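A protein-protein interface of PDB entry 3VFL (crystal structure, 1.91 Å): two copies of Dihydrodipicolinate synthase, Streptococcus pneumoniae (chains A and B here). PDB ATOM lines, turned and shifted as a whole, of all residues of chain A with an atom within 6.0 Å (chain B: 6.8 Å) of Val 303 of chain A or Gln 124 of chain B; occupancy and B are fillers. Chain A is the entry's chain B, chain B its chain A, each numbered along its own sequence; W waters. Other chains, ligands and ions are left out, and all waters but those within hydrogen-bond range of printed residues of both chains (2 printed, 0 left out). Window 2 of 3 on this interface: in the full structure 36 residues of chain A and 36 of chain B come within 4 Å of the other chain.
The side-chain amide oxygen of Gln 124 of chain B lies within hydrogen-bond range of the backbone NH of Gly 305 of chain A (3.2 Å).
The side-chain amide nitrogen (NE2) of Gln 124 of chain B sits at hydrogen-bond distance from the backbone carbonyl oxygen (O) of Val 303 of chain A, at 2.8 Å.
The side-chain hydroxyl (OG1) of Thr 88 of chain B sits close to the backbone carbonyl oxygen (O) of Leu 274 of chain A, at 3.3 Å.
Of the 15 printed residues of chain B, 4 touch a printed residue of chain A.
Along chain B the printed residues that touch a printed residue of chain A span positions 88 to 124.
Printed residues of chain A that touch a printed residue of chain B: Tyr 252, Leu 274, Val 277, Val 303, Thr 304 and Gly 305.
Hydrophobic or aromatic side chains of chain A that line the printed part of chain B: Tyr 252, Leu 274 and Val 277.
Among the printed residues, no Asp or Glu carboxylate lies within 4 Å of a Lys or Arg side-chain nitrogen of the other chain.
Among the printed residues, merely in contact across the chains: Tyr 252 of chain A with Glu 120 of chain B (3.8 Å), Leu 274 of chain A with Gln 124 of chain B (3.7 Å), Val 277 of chain A with Glu 120 of chain B (3.8 Å), Val 277 of chain A with Gly 121 of chain B (3.7 Å), Val 277 of chain A with Gln 124 of chain B (3.5 Å) and Thr 304 of chain A with Gln 124 of chain B (3.9 Å).
No position is printed for both chains.
Water W1 lies within hydrogen-bond range of O of Leu 274 of chain A and N of Thr 88 of chain B.
Water W2 lies within hydrogen-bond range of the backbone NH of Glu 120 of chain B, the side-chain hydroxyl of Tyr 252 of chain A and the backbone NH of Gln 119 of chain B.
Val 303 of chain A touches just one residue of chain B: Gln 124.
Gln 124 of chain B touches just these residues of chain A: Leu 274 (3.7 Å), Val 277 (3.5 Å), Val 303 (2.8 Å), Thr 304 (3.9 Å) and Gly 305 (3.2 Å).
Of the printed residues of chain B, Gly 305 of chain A touches Gln 124.
Of the printed residues of chain A, Thr 88 of chain B touches Leu 274.
Of the printed residues of chain A, Glu 120 of chain B touches Tyr 252 and Val 277.
Of the printed residues of chain B, Tyr 252 of chain A touches Glu 120.
Of the printed residues of chain B, Val 277 of chain A touches Glu 120, Gly 121 and Gln 124.
Ala 128 of chain B touches none of the printed residues of chain A.
Met 122 of chain B touches none of the printed residues of chain A.
OE1 of Glu 120 of chain B is in salt-bridge range of NH2 of Arg 157 of chain B, 3.8 Å away.
The side-chain carboxylate (OE2) of Glu 120 of chain B sits at hydrogen-bond distance from the side-chain amide nitrogen (NE2) of Gln 124 of chain B, at 3.0 Å.
OG1 of Thr 88 of chain B is in hydrogen-bond range of ND1 of His 125 of chain B (2.8 Å).
N of Leu 274 of chain A lies within hydrogen-bond range of O of Val 306 of chain A (2.9 Å).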
ATOM      1  N   TYR A 252     -26.143 -20.738  -1.901  1.00  0.00           N
ATOM      2  CA  TYR A 252     -25.638 -20.547  -0.564  1.00  0.00           C
ATOM      3  C   TYR A 252     -25.524 -21.995  -0.206  1.00  0.00           C
ATOM      4  O   TYR A 252     -26.178 -22.836  -0.820  1.00  0.00           O
ATOM      5  CB  TYR A 252     -26.629 -19.714   0.367  1.00  0.00           C
ATOM      6  CG  TYR A 252     -25.963 -19.144   1.620  1.00  0.00           C
ATOM      7  CD1 TYR A 252     -25.122 -18.021   1.542  1.00  0.00           C
ATOM      8  CD2 TYR A 252     -26.135 -19.750   2.859  1.00  0.00           C
ATOM      9  CE1 TYR A 252     -24.461 -17.567   2.661  1.00  0.00           C
ATOM     10  CE2 TYR A 252     -25.476 -19.300   3.992  1.00  0.00           C
ATOM     11  CZ  TYR A 252     -24.681 -18.217   3.882  1.00  0.00           C
ATOM     12  OH  TYR A 252     -24.029 -17.767   4.947  1.00  0.00           O
ATOM     13  N   LEU A 274     -25.364 -25.707  12.646  1.00  0.00           N
ATOM     14  CA  LEU A 274     -23.936 -25.251  12.556  1.00  0.00           C
ATOM     15  C   LEU A 274     -23.000 -26.504  12.285  1.00  0.00           C
ATOM     16  O   LEU A 274     -23.181 -27.547  12.897  1.00  0.00           O
ATOM     17  CB  LEU A 274     -23.557 -24.451  13.823  1.00  0.00           C
ATOM     18  CG  LEU A 274     -24.132 -23.020  13.950  1.00  0.00           C
ATOM     19  CD1 LEU A 274     -23.624 -22.371  15.229  1.00  0.00           C
ATOM     20  CD2 LEU A 274     -23.775 -22.141  12.764  1.00  0.00           C
ATOM     21  N   VAL A 277     -25.240 -22.223   8.060  1.00  0.00           N
ATOM     22  CA  VAL A 277     -26.219 -21.204   8.503  1.00  0.00           C
ATOM     23  C   VAL A 277     -27.253 -21.044   7.430  1.00  0.00           C
ATOM     24  O   VAL A 277     -26.970 -21.308   6.242  1.00  0.00           O
ATOM     25  CB  VAL A 277     -25.604 -19.829   8.810  1.00  0.00           C
ATOM     26  CG1 VAL A 277     -24.825 -19.869  10.144  1.00  0.00           C
ATOM     27  CG2 VAL A 277     -24.688 -19.345   7.710  1.00  0.00           C
ATOM     28  N   PRO A 278     -28.470 -20.572   7.826  1.00  0.00           N
ATOM     29  CA  PRO A 278     -29.503 -20.455   6.806  1.00  0.00           C
ATOM     30  C   PRO A 278     -29.107 -19.449   5.739  1.00  0.00           C
ATOM     31  O   PRO A 278     -28.167 -18.614   5.939  1.00  0.00           O
ATOM     32  CB  PRO A 278     -30.749 -19.973   7.627  1.00  0.00           C
ATOM     33  CG  PRO A 278     -30.537 -20.551   9.000  1.00  0.00           C
ATOM     34  CD  PRO A 278     -29.026 -20.462   9.204  1.00  0.00           C
ATOM     35  N   ALA A 279     -29.773 -19.515   4.593  1.00  0.00           N
ATOM     36  CA  ALA A 279     -29.566 -18.482   3.573  1.00  0.00           C
ATOM     37  C   ALA A 279     -29.827 -17.042   4.070  1.00  0.00           C
ATOM     38  O   ALA A 279     -30.856 -16.803   4.661  1.00  0.00           O
ATOM     39  CB  ALA A 279     -30.474 -18.782   2.390  1.00  0.00           C
ATOM     40  N   PRO A 280     -28.934 -16.067   3.787  1.00  0.00           N
ATOM     41  CA  PRO A 280     -29.260 -14.672   4.155  1.00  0.00           C
ATOM     42  C   PRO A 280     -30.551 -14.121   3.499  1.00  0.00           C
ATOM     43  O   PRO A 280     -30.994 -14.584   2.405  1.00  0.00           O
ATOM     44  CB  PRO A 280     -28.022 -13.887   3.719  1.00  0.00           C
ATOM     45  CG  PRO A 280     -26.938 -14.912   3.587  1.00  0.00           C
ATOM     46  CD  PRO A 280     -27.646 -16.144   3.075  1.00  0.00           C
ATOM     47  N   GLU A 281     -31.160 -13.142   4.171  1.00  0.00           N
ATOM     48  CA  GLU A 281     -32.477 -12.591   3.794  1.00  0.00           C
ATOM     49  C   GLU A 281     -32.606 -12.172   2.312  1.00  0.00           C
ATOM     50  O   GLU A 281     -33.509 -12.625   1.618  1.00  0.00           O
ATOM     51  CB  GLU A 281     -32.765 -11.368   4.692  1.00  0.00           C
ATOM     52  CG  GLU A 281     -34.187 -11.155   5.210  1.00  0.00           C
ATOM     53  CD  GLU A 281     -34.269  -9.957   6.197  1.00  0.00           C
ATOM     54  OE1 GLU A 281     -33.283  -9.725   6.972  1.00  0.00           O
ATOM     55  OE2 GLU A 281     -35.316  -9.235   6.219  1.00  0.00           O
ATOM     56  N   THR A 302     -28.946 -10.551  10.700  1.00  0.00           N
ATOM     57  CA  THR A 302     -28.204 -11.728  10.197  1.00  0.00           C
ATOM     58  C   THR A 302     -28.720 -13.077  10.684  1.00  0.00           C
ATOM     59  O   THR A 302     -29.461 -13.211  11.657  1.00  0.00           O
ATOM     60  CB  THR A 302     -26.735 -11.748  10.628  1.00  0.00           C
ATOM     61  OG1 THR A 302     -26.202 -13.045  10.254  1.00  0.00           O
ATOM     62  CG2 THR A 302     -26.631 -11.587  12.129  1.00  0.00           C
ATOM     63  N   VAL A 303     -28.171 -14.087  10.044  1.00  0.00           N
ATOM     64  CA  VAL A 303     -28.772 -15.382   9.926  1.00  0.00           C
ATOM     65  C   VAL A 303     -28.180 -16.268  11.028  1.00  0.00           C
ATOM     66  O   VAL A 303     -27.045 -16.058  11.459  1.00  0.00           O
ATOM     67  CB  VAL A 303     -28.393 -15.867   8.525  1.00  0.00           C
ATOM     68  CG1 VAL A 303     -29.193 -17.067   8.147  1.00  0.00           C
ATOM     69  CG2 VAL A 303     -28.593 -14.741   7.509  1.00  0.00           C
ATOM     70  N   THR A 304     -28.924 -17.265  11.488  1.00  0.00           N
ATOM     71  CA  THR A 304     -28.523 -17.953  12.715  1.00  0.00           C
ATOM     72  C   THR A 304     -28.607 -19.450  12.551  1.00  0.00           C
ATOM     73  O   THR A 304     -29.692 -20.004  12.334  1.00  0.00           O
ATOM     74  CB  THR A 304     -29.387 -17.447  13.900  1.00  0.00           C
ATOM     75  OG1 THR A 304     -28.897 -16.177  14.312  1.00  0.00           O
ATOM     76  CG2 THR A 304     -29.373 -18.388  15.076  1.00  0.00           C
ATOM     77  N   GLY A 305     -27.457 -20.119  12.592  1.00  0.00           N
ATOM     78  CA  GLY A 305     -27.428 -21.586  12.525  1.00  0.00           C
ATOM     79  C   GLY A 305     -27.622 -22.086  13.942  1.00  0.00           C
ATOM     80  O   GLY A 305     -27.318 -21.359  14.887  1.00  0.00           O
ATOM     81  N   VAL A 306     -28.083 -23.321  14.128  1.00  0.00           N
ATOM     82  CA  VAL A 306     -28.518 -23.720  15.440  1.00  0.00           C
ATOM     83  C   VAL A 306     -27.655 -24.911  15.892  1.00  0.00           C
ATOM     84  O   VAL A 306     -26.959 -25.548  15.068  1.00  0.00           O
ATOM     85  CB  VAL A 306     -30.047 -24.009  15.480  1.00  0.00           C
ATOM     86  CG1 VAL A 306     -30.860 -22.802  14.888  1.00  0.00           C
ATOM     87  CG2 VAL A 306     -30.375 -25.255  14.666  1.00  0.00           C
ATOM     88  N   THR B  88     -20.350 -28.635  14.906  1.00  0.00           N
ATOM     89  CA  THR B  88     -20.057 -27.623  15.904  1.00  0.00           C
ATOM     90  C   THR B  88     -20.350 -28.085  17.369  1.00  0.00           C
ATOM     91  O   THR B  88     -19.503 -27.930  18.259  1.00  0.00           O
ATOM     92  CB  THR B  88     -20.819 -26.352  15.617  1.00  0.00           C
ATOM     93  OG1 THR B  88     -20.622 -25.960  14.262  1.00  0.00           O
ATOM     94  CG2 THR B  88     -20.294 -25.198  16.554  1.00  0.00           C
ATOM     95  N   GLN B 119     -18.694 -18.450   4.869  1.00  0.00           N
ATOM     96  CA  GLN B 119     -17.871 -17.707   5.785  1.00  0.00           C
ATOM     97  C   GLN B 119     -18.663 -17.463   7.115  1.00  0.00           C
ATOM     98  O   GLN B 119     -18.099 -17.536   8.207  1.00  0.00           O
ATOM     99  CB  GLN B 119     -17.423 -16.334   5.215  1.00  0.00           C
ATOM    100  CG  GLN B 119     -16.591 -16.371   3.991  1.00  0.00           C
ATOM    101  CD  GLN B 119     -15.380 -17.288   4.162  1.00  0.00           C
ATOM    102  OE1 GLN B 119     -15.302 -18.350   3.507  1.00  0.00           O
ATOM    103  NE2 GLN B 119     -14.472 -16.928   5.041  1.00  0.00           N
ATOM    104  N   GLU B 120     -19.954 -17.187   7.012  1.00  0.00           N
ATOM    105  CA  GLU B 120     -20.718 -16.860   8.273  1.00  0.00           C
ATOM    106  C   GLU B 120     -20.829 -18.094   9.061  1.00  0.00           C
ATOM    107  O   GLU B 120     -20.775 -18.083  10.324  1.00  0.00           O
ATOM    108  CB  GLU B 120     -22.173 -16.448   7.969  1.00  0.00           C
ATOM    109  CG  GLU B 120     -22.974 -16.116   9.265  1.00  0.00           C
ATOM    110  CD  GLU B 120     -22.324 -14.959  10.073  1.00  0.00           C
ATOM    111  OE1 GLU B 120     -21.512 -14.224   9.471  1.00  0.00           O
ATOM    112  OE2 GLU B 120     -22.592 -14.764  11.294  1.00  0.00           O
ATOM    113  N   GLY B 121     -21.055 -19.194   8.322  1.00  0.00           N
ATOM    114  CA  GLY B 121     -21.109 -20.489   8.949  1.00  0.00           C
ATOM    115  C   GLY B 121     -19.838 -20.806   9.726  1.00  0.00           C
ATOM    116  O   GLY B 121     -19.901 -21.161  10.914  1.00  0.00           O
ATOM    117  N   MET B 122     -18.673 -20.625   9.083  1.00  0.00           N
ATOM    118  CA  MET B 122     -17.389 -20.892   9.733  1.00  0.00           C
ATOM    119  C   MET B 122     -17.221 -19.989  10.952  1.00  0.00           C
ATOM    120  O   MET B 122     -16.719 -20.447  11.962  1.00  0.00           O
ATOM    121  CB  MET B 122     -16.190 -20.667   8.783  1.00  0.00           C
ATOM    122  CG  MET B 122     -16.243 -21.401   7.419  1.00  0.00           C
ATOM    123  SD  MET B 122     -14.942 -20.856   6.263  1.00  0.00           S
ATOM    124  CE  MET B 122     -15.514 -21.658   4.756  1.00  0.00           C
ATOM    125  N   TYR B 123     -17.625 -18.719  10.812  1.00  0.00           N
ATOM    126  CA  TYR B 123     -17.473 -17.672  11.832  1.00  0.00           C
ATOM    127  C   TYR B 123     -18.232 -18.129  13.095  1.00  0.00           C
ATOM    128  O   TYR B 123     -17.626 -18.294  14.187  1.00  0.00           O
ATOM    129  CB  TYR B 123     -17.997 -16.281  11.331  1.00  0.00           C
ATOM    130  CG  TYR B 123     -17.969 -15.254  12.482  1.00  0.00           C
ATOM    131  CD1 TYR B 123     -16.773 -14.630  12.833  1.00  0.00           C
ATOM    132  CD2 TYR B 123     -19.116 -14.995  13.271  1.00  0.00           C
ATOM    133  CE1 TYR B 123     -16.694 -13.740  13.892  1.00  0.00           C
ATOM    134  CE2 TYR B 123     -19.036 -14.119  14.350  1.00  0.00           C
ATOM    135  CZ  TYR B 123     -17.829 -13.511  14.658  1.00  0.00           C
ATOM    136  OH  TYR B 123     -17.695 -12.637  15.709  1.00  0.00           O
ATOM    137  N   GLN B 124     -19.536 -18.389  12.922  1.00  0.00           N
ATOM    138  CA  GLN B 124     -20.417 -18.883  14.007  1.00  0.00           C
ATOM    139  C   GLN B 124     -19.900 -20.196  14.554  1.00  0.00           C
ATOM    140  O   GLN B 124     -19.953 -20.401  15.763  1.00  0.00           O
ATOM    141  CB  GLN B 124     -21.891 -19.023  13.594  1.00  0.00           C
ATOM    142  CG  GLN B 124     -22.579 -17.700  13.335  1.00  0.00           C
ATOM    143  CD  GLN B 124     -24.055 -17.819  12.999  1.00  0.00           C
ATOM    144  OE1 GLN B 124     -24.789 -18.653  13.555  1.00  0.00           O
ATOM    145  NE2 GLN B 124     -24.487 -17.019  12.072  1.00  0.00           N
ATOM    146  N   HIS B 125     -19.370 -21.073  13.698  1.00  0.00           N
ATOM    147  CA  HIS B 125     -18.685 -22.340  14.141  1.00  0.00           C
ATOM    148  C   HIS B 125     -17.556 -22.057  15.092  1.00  0.00           C
ATOM    149  O   HIS B 125     -17.523 -22.627  16.179  1.00  0.00           O
ATOM    150  CB  HIS B 125     -18.156 -23.142  12.943  1.00  0.00           C
ATOM    151  CG  HIS B 125     -17.371 -24.394  13.275  1.00  0.00           C
ATOM    152  ND1 HIS B 125     -17.955 -25.498  13.724  1.00  0.00           N
ATOM    153  CD2 HIS B 125     -16.000 -24.709  13.124  1.00  0.00           C
ATOM    154  CE1 HIS B 125     -17.045 -26.472  13.903  1.00  0.00           C
ATOM    155  NE2 HIS B 125     -15.849 -26.007  13.475  1.00  0.00           N
ATOM    156  N   PHE B 126     -16.608 -21.218  14.722  1.00  0.00           N
ATOM    157  CA  PHE B 126     -15.416 -21.220  15.500  1.00  0.00           C
ATOM    158  C   PHE B 126     -15.664 -20.376  16.744  1.00  0.00           C
ATOM    159  O   PHE B 126     -14.975 -20.599  17.736  1.00  0.00           O
ATOM    160  CB  PHE B 126     -14.231 -20.625  14.772  1.00  0.00           C
ATOM    161  CG  PHE B 126     -13.647 -21.522  13.747  1.00  0.00           C
ATOM    162  CD1 PHE B 126     -12.879 -22.603  14.116  1.00  0.00           C
ATOM    163  CD2 PHE B 126     -13.877 -21.271  12.385  1.00  0.00           C
ATOM    164  CE1 PHE B 126     -12.325 -23.446  13.143  1.00  0.00           C
ATOM    165  CE2 PHE B 126     -13.336 -22.105  11.444  1.00  0.00           C
ATOM    166  CZ  PHE B 126     -12.535 -23.164  11.815  1.00  0.00           C
ATOM    167  N   LYS B 127     -16.574 -19.413  16.617  1.00  0.00           N
ATOM    168  CA  LYS B 127     -17.000 -18.543  17.744  1.00  0.00           C
ATOM    169  C   LYS B 127     -17.535 -19.455  18.841  1.00  0.00           C
ATOM    170  O   LYS B 127     -17.130 -19.336  19.967  1.00  0.00           O
ATOM    171  CB  LYS B 127     -18.040 -17.497  17.313  1.00  0.00           C
ATOM    172  CG  LYS B 127     -18.658 -16.621  18.446  1.00  0.00           C
ATOM    173  CD  LYS B 127     -19.849 -15.817  17.917  1.00  0.00           C
ATOM    174  CE  LYS B 127     -19.995 -14.452  18.589  1.00  0.00           C
ATOM    175  NZ  LYS B 127     -20.230 -14.501  20.073  1.00  0.00           N
ATOM    176  N   ALA B 128     -18.401 -20.392  18.463  1.00  0.00           N
ATOM    177  CA  ALA B 128     -19.016 -21.281  19.407  1.00  0.00           C
ATOM    178  C   ALA B 128     -17.989 -22.151  20.103  1.00  0.00           C
ATOM    179  O   ALA B 128     -18.105 -22.371  21.305  1.00  0.00           O
ATOM    180  CB  ALA B 128     -20.103 -22.150  18.771  1.00  0.00           C
ATOM    181  N   ILE B 129     -16.975 -22.629  19.384  1.00  0.00           N
ATOM    182  CA  ILE B 129     -15.939 -23.430  19.983  1.00  0.00           C
ATOM    183  C   ILE B 129     -14.981 -22.617  20.857  1.00  0.00           C
ATOM    184  O   ILE B 129     -14.476 -23.153  21.863  1.00  0.00           O
ATOM    185  CB  ILE B 129     -15.130 -24.212  18.898  1.00  0.00           C
ATOM    186  CG1 ILE B 129     -16.055 -25.099  18.057  1.00  0.00           C
ATOM    187  CG2 ILE B 129     -14.038 -25.095  19.514  1.00  0.00           C
ATOM    188  CD1 ILE B 129     -15.418 -25.616  16.759  1.00  0.00           C
ATOM    189  N   ASP B 131     -15.977 -19.944  22.370  1.00  0.00           N
ATOM    190  CA  ASP B 131     -16.807 -19.516  23.501  1.00  0.00           C
ATOM    191  C   ASP B 131     -16.849 -20.592  24.552  1.00  0.00           C
ATOM    192  O   ASP B 131     -16.956 -20.303  25.727  1.00  0.00           O
ATOM    193  CB  ASP B 131     -18.234 -19.185  23.039  1.00  0.00           C
ATOM    194  CG  ASP B 131     -18.388 -17.788  22.486  1.00  0.00           C
ATOM    195  OD1 ASP B 131     -17.578 -16.872  22.694  1.00  0.00           O
ATOM    196  OD2 ASP B 131     -19.413 -17.564  21.823  1.00  0.00           O
ATOM    197  N   ARG B 157     -11.554 -11.387  11.539  1.00  0.00           N
ATOM    198  CA  ARG B 157     -12.725 -11.268  12.446  1.00  0.00           C
ATOM    199  C   ARG B 157     -12.584 -12.216  13.646  1.00  0.00           C
ATOM    200  O   ARG B 157     -12.795 -11.802  14.805  1.00  0.00           O
ATOM    201  CB  ARG B 157     -14.057 -11.518  11.719  1.00  0.00           C
ATOM    202  CG  ARG B 157     -14.723 -10.257  11.182  1.00  0.00           C
ATOM    203  CD  ARG B 157     -15.923 -10.620  10.297  1.00  0.00           C
ATOM    204  NE  ARG B 157     -17.065 -11.094  11.106  1.00  0.00           N
ATOM    205  CZ  ARG B 157     -17.987 -11.981  10.715  1.00  0.00           C
ATOM    206  NH1 ARG B 157     -17.939 -12.551   9.499  1.00  0.00           N
ATOM    207  NH2 ARG B 157     -18.946 -12.318  11.563  1.00  0.00           N
ATOM    208  N   LEU B 158     -12.107 -13.442  13.416  1.00  0.00           N
ATOM    209  CA  LEU B 158     -12.064 -14.389  14.456  1.00  0.00           C
ATOM    210  C   LEU B 158     -10.916 -14.139  15.411  1.00  0.00           C
ATOM    211  O   LEU B 158     -11.085 -14.340  16.612  1.00  0.00           O
ATOM    212  CB  LEU B 158     -12.072 -15.837  13.906  1.00  0.00           C
ATOM    213  CG  LEU B 158     -13.387 -16.431  13.413  1.00  0.00           C
ATOM    214  CD1 LEU B 158     -13.067 -17.746  12.682  1.00  0.00           C
ATOM    215  CD2 LEU B 158     -14.363 -16.739  14.573  1.00  0.00           C
HETATM  216  O   HOH W   1     -23.473 -28.369  15.181  1.00  0.00           O
HETATM  217  O   HOH W   2     -21.195 -16.184   4.556  1.00  0.00           O
